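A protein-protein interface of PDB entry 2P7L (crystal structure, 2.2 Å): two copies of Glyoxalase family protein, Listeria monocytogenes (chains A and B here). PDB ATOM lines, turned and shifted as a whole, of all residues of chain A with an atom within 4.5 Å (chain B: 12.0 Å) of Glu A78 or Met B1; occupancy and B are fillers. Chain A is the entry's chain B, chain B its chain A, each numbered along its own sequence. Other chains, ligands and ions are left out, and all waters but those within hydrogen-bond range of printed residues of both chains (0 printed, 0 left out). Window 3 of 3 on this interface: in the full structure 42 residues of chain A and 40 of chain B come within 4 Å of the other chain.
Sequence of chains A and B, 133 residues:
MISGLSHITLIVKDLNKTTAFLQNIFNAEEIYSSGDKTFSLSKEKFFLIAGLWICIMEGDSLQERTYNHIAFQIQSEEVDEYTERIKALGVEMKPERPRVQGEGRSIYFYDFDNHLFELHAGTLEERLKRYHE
OG of Ser B3 is in hydrogen-bond range of NE2 of Gln A75, 3.1 Å away.
OH of Tyr A82 lies close to N of Met B1 (3.1 Å).
N of Met B1 lies within hydrogen-bond range of OE1 of Glu A78, 3.3 Å away.
Of the 6 printed residues of chain B, 3 touch a printed residue of chain A.
Hydrophobic or aromatic side chains of chain A within 4 Å of the printed part of chain B: Tyr A82.
Among the printed residues, 5 pairs touch across the chains.
Among the printed residues, no Asp or Glu carboxylate lies within 4 Å of a Lys or Arg side-chain nitrogen of the other chain.
Of chain B, only Met B1 (3.3 Å) comes within 4 Å of Glu A78.
Met B1 touches just these residues of chain A: Asn A27, Glu A78 and Tyr A82.
Asn A27 touches just one residue of chain B: Met B1 (3.9 Å).
Of chain B, only Ser B3 comes within 4 Å of Gln A75.
No residue of chain B comes within 4 Å of Glu A77.
No residue of chain B comes within 4 Å of Val A79.
No residue of chain B comes within 4 Å of Asp A80.
Tyr A82 touches just these residues of chain B: Met B1 (3.1 Å) and Ile B2 (3.6 Å).
Of the printed residues of chain A, Ser B3 touches Gln A75.
Of the printed residues of chain A, Ile B2 touches Tyr A82.
The nearest residue of chain B that does not touch Glu A78 is Ser B3 (5.3 Å).
The nearest printed residue of chain A that does not touch Ser B3 is Ile A74 (4.3 Å).
The backbone NH (N) of Gln A75 sits close to the side-chain carboxylate (OE2) of Glu A78 (3.3 Å).
No position is printed for both chains.
Asn A27 touches Met B1 (ND2 to CA, 3.9 Å).
N of Ile B2 touches OH of Tyr A82, 3.6 Å away.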
ATOM      1  N   ASN A  27      14.602 -11.669 -20.864  1.00  0.00           N
ATOM      2  CA  ASN A  27      15.001 -12.916 -21.516  1.00  0.00           C
ATOM      3  C   ASN A  27      15.320 -13.911 -20.408  1.00  0.00           C
ATOM      4  O   ASN A  27      16.209 -14.740 -20.549  1.00  0.00           O
ATOM      5  CB  ASN A  27      16.270 -12.737 -22.365  1.00  0.00           C
ATOM      6  CG  ASN A  27      16.073 -11.800 -23.536  1.00  0.00           C
ATOM      7  OD1 ASN A  27      15.080 -11.893 -24.258  1.00  0.00           O
ATOM      8  ND2 ASN A  27      17.033 -10.900 -23.746  1.00  0.00           N
ATOM      9  N   ILE A  74      22.505  -2.443 -19.461  1.00  0.00           N
ATOM     10  CA  ILE A  74      22.229  -2.567 -20.893  1.00  0.00           C
ATOM     11  C   ILE A  74      23.116  -1.559 -21.630  1.00  0.00           C
ATOM     12  O   ILE A  74      24.029  -0.987 -21.037  1.00  0.00           O
ATOM     13  CB  ILE A  74      20.742  -2.261 -21.230  1.00  0.00           C
ATOM     14  CG1 ILE A  74      20.384  -0.837 -20.793  1.00  0.00           C
ATOM     15  CG2 ILE A  74      19.830  -3.279 -20.560  1.00  0.00           C
ATOM     16  CD1 ILE A  74      18.972  -0.421 -21.168  1.00  0.00           C
ATOM     17  N   GLN A  75      22.852  -1.338 -22.914  1.00  0.00           N
ATOM     18  CA  GLN A  75      23.639  -0.381 -23.691  1.00  0.00           C
ATOM     19  C   GLN A  75      22.842   0.894 -23.953  1.00  0.00           C
ATOM     20  O   GLN A  75      21.608   0.891 -23.929  1.00  0.00           O
ATOM     21  CB  GLN A  75      24.053  -0.987 -25.028  1.00  0.00           C
ATOM     22  CG  GLN A  75      24.657  -2.374 -24.918  1.00  0.00           C
ATOM     23  CD  GLN A  75      25.882  -2.402 -24.040  1.00  0.00           C
ATOM     24  OE1 GLN A  75      26.911  -1.807 -24.369  1.00  0.00           O
ATOM     25  NE2 GLN A  75      25.781  -3.095 -22.906  1.00  0.00           N
ATOM     26  N   SER A  76      23.549   1.988 -24.198  1.00  0.00           N
ATOM     27  CA  SER A  76      22.884   3.249 -24.472  1.00  0.00           C
ATOM     28  C   SER A  76      22.048   3.090 -25.730  1.00  0.00           C
ATOM     29  O   SER A  76      20.927   3.596 -25.817  1.00  0.00           O
ATOM     30  CB  SER A  76      23.915   4.352 -24.681  1.00  0.00           C
ATOM     31  OG  SER A  76      24.746   4.470 -23.546  1.00  0.00           O
ATOM     32  N   GLU A  77      22.603   2.373 -26.703  1.00  0.00           N
ATOM     33  CA  GLU A  77      21.927   2.151 -27.973  1.00  0.00           C
ATOM     34  C   GLU A  77      20.628   1.375 -27.791  1.00  0.00           C
ATOM     35  O   GLU A  77      19.727   1.442 -28.634  1.00  0.00           O
ATOM     36  CB  GLU A  77      22.831   1.375 -28.936  1.00  0.00           C
ATOM     37  CG  GLU A  77      24.298   1.768 -28.905  1.00  0.00           C
ATOM     38  CD  GLU A  77      25.120   0.903 -27.953  1.00  0.00           C
ATOM     39  OE1 GLU A  77      25.070  -0.342 -28.086  1.00  0.00           O
ATOM     40  OE2 GLU A  77      25.822   1.462 -27.082  1.00  0.00           O
ATOM     41  N   GLU A  78      20.527   0.645 -26.685  1.00  0.00           N
ATOM     42  CA  GLU A  78      19.343  -0.157 -26.431  1.00  0.00           C
ATOM     43  C   GLU A  78      18.324   0.500 -25.521  1.00  0.00           C
ATOM     44  O   GLU A  78      17.295  -0.104 -25.216  1.00  0.00           O
ATOM     45  CB  GLU A  78      19.744  -1.500 -25.832  1.00  0.00           C
ATOM     46  CG  GLU A  78      20.958  -2.127 -26.483  1.00  0.00           C
ATOM     47  CD  GLU A  78      21.212  -3.534 -25.985  1.00  0.00           C
ATOM     48  OE1 GLU A  78      20.595  -4.474 -26.532  1.00  0.00           O
ATOM     49  OE2 GLU A  78      22.016  -3.695 -25.040  1.00  0.00           O
ATOM     50  N   VAL A  79      18.589   1.725 -25.084  1.00  0.00           N
ATOM     51  CA  VAL A  79      17.648   2.395 -24.194  1.00  0.00           C
ATOM     52  C   VAL A  79      16.267   2.605 -24.807  1.00  0.00           C
ATOM     53  O   VAL A  79      15.263   2.191 -24.227  1.00  0.00           O
ATOM     54  CB  VAL A  79      18.186   3.763 -23.708  1.00  0.00           C
ATOM     55  CG1 VAL A  79      17.070   4.529 -23.003  1.00  0.00           C
ATOM     56  CG2 VAL A  79      19.363   3.550 -22.753  1.00  0.00           C
ATOM     57  N   ASP A  80      16.211   3.266 -25.962  1.00  0.00           N
ATOM     58  CA  ASP A  80      14.933   3.511 -26.628  1.00  0.00           C
ATOM     59  C   ASP A  80      14.196   2.182 -26.780  1.00  0.00           C
ATOM     60  O   ASP A  80      13.001   2.090 -26.507  1.00  0.00           O
ATOM     61  CB  ASP A  80      15.142   4.142 -28.016  1.00  0.00           C
ATOM     62  CG  ASP A  80      15.859   5.484 -27.957  1.00  0.00           C
ATOM     63  OD1 ASP A  80      15.576   6.282 -27.033  1.00  0.00           O
ATOM     64  OD2 ASP A  80      16.695   5.752 -28.852  1.00  0.00           O
ATOM     65  N   GLU A  81      14.928   1.155 -27.205  1.00  0.00           N
ATOM     66  CA  GLU A  81      14.362  -0.181 -27.400  1.00  0.00           C
ATOM     67  C   GLU A  81      13.628  -0.714 -26.157  1.00  0.00           C
ATOM     68  O   GLU A  81      12.431  -1.018 -26.215  1.00  0.00           O
ATOM     69  CB  GLU A  81      15.469  -1.165 -27.802  1.00  0.00           C
ATOM     70  CG  GLU A  81      15.010  -2.605 -27.909  1.00  0.00           C
ATOM     71  CD  GLU A  81      16.146  -3.604 -27.739  1.00  0.00           C
ATOM     72  OE1 GLU A  81      17.300  -3.254 -28.060  1.00  0.00           O
ATOM     73  OE2 GLU A  81      15.885  -4.744 -27.297  1.00  0.00           O
ATOM     74  N   TYR A  82      14.342  -0.833 -25.039  1.00  0.00           N
ATOM     75  CA  TYR A  82      13.723  -1.344 -23.820  1.00  0.00           C
ATOM     76  C   TYR A  82      12.604  -0.450 -23.308  1.00  0.00           C
ATOM     77  O   TYR A  82      11.634  -0.925 -22.717  1.00  0.00           O
ATOM     78  CB  TYR A  82      14.766  -1.552 -22.729  1.00  0.00           C
ATOM     79  CG  TYR A  82      15.541  -2.835 -22.892  1.00  0.00           C
ATOM     80  CD1 TYR A  82      16.801  -2.843 -23.473  1.00  0.00           C
ATOM     81  CD2 TYR A  82      14.989  -4.056 -22.494  1.00  0.00           C
ATOM     82  CE1 TYR A  82      17.497  -4.040 -23.656  1.00  0.00           C
ATOM     83  CE2 TYR A  82      15.673  -5.252 -22.678  1.00  0.00           C
ATOM     84  CZ  TYR A  82      16.925  -5.236 -23.258  1.00  0.00           C
ATOM     85  OH  TYR A  82      17.610  -6.417 -23.435  1.00  0.00           O
ATOM     86  N   MET B   1      19.972  -7.390 -25.178  1.00  0.00           N
ATOM     87  CA  MET B   1      19.943  -8.322 -24.012  1.00  0.00           C
ATOM     88  C   MET B   1      20.563  -7.683 -22.767  1.00  0.00           C
ATOM     89  O   MET B   1      21.356  -6.745 -22.862  1.00  0.00           O
ATOM     90  CB  MET B   1      20.711  -9.609 -24.341  1.00  0.00           C
ATOM     91  CG  MET B   1      22.192  -9.376 -24.652  1.00  0.00           C
ATOM     92  SD  MET B   1      23.253 -10.843 -24.443  1.00  0.00           S
ATOM     93  CE  MET B   1      24.172 -10.397 -22.940  1.00  0.00           C
ATOM     94  N   ILE B   2      20.198  -8.202 -21.601  1.00  0.00           N
ATOM     95  CA  ILE B   2      20.738  -7.710 -20.341  1.00  0.00           C
ATOM     96  C   ILE B   2      22.180  -8.202 -20.253  1.00  0.00           C
ATOM     97  O   ILE B   2      22.434  -9.400 -20.381  1.00  0.00           O
ATOM     98  CB  ILE B   2      19.953  -8.283 -19.144  1.00  0.00           C
ATOM     99  CG1 ILE B   2      18.444  -8.140 -19.383  1.00  0.00           C
ATOM    100  CG2 ILE B   2      20.373  -7.587 -17.869  1.00  0.00           C
ATOM    101  CD1 ILE B   2      17.986  -6.732 -19.664  1.00  0.00           C
ATOM    102  N   SER B   3      23.122  -7.287 -20.043  1.00  0.00           N
ATOM    103  CA  SER B   3      24.541  -7.655 -19.951  1.00  0.00           C
ATOM    104  C   SER B   3      24.846  -8.319 -18.623  1.00  0.00           C
ATOM    105  O   SER B   3      25.713  -9.184 -18.528  1.00  0.00           O
ATOM    106  CB  SER B   3      25.434  -6.415 -20.083  1.00  0.00           C
ATOM    107  OG  SER B   3      25.130  -5.668 -21.252  1.00  0.00           O
ATOM    108  N   GLY B   4      24.131  -7.888 -17.594  1.00  0.00           N
ATOM    109  CA  GLY B   4      24.333  -8.427 -16.263  1.00  0.00           C
ATOM    110  C   GLY B   4      23.813  -7.448 -15.229  1.00  0.00           C
ATOM    111  O   GLY B   4      23.025  -6.552 -15.546  1.00  0.00           O
ATOM    112  N   LEU B   5      24.257  -7.610 -13.991  1.00  0.00           N
ATOM    113  CA  LEU B   5      23.831  -6.734 -12.907  1.00  0.00           C
ATOM    114  C   LEU B   5      24.641  -5.437 -12.900  1.00  0.00           C
ATOM    115  O   LEU B   5      25.867  -5.471 -12.959  1.00  0.00           O
ATOM    116  CB  LEU B   5      24.003  -7.465 -11.574  1.00  0.00           C
ATOM    117  CG  LEU B   5      23.553  -6.825 -10.261  1.00  0.00           C
ATOM    118  CD1 LEU B   5      22.057  -6.582 -10.279  1.00  0.00           C
ATOM    119  CD2 LEU B   5      23.916  -7.759  -9.111  1.00  0.00           C
ATOM    120  N   SER B   6      23.959  -4.299 -12.855  1.00  0.00           N
ATOM    121  CA  SER B   6      24.648  -3.010 -12.804  1.00  0.00           C
ATOM    122  C   SER B   6      24.997  -2.687 -11.355  1.00  0.00           C
ATOM    123  O   SER B   6      26.169  -2.533 -11.007  1.00  0.00           O
ATOM    124  CB  SER B   6      23.769  -1.884 -13.348  1.00  0.00           C
ATOM    125  OG  SER B   6      24.408  -0.627 -13.162  1.00  0.00           O
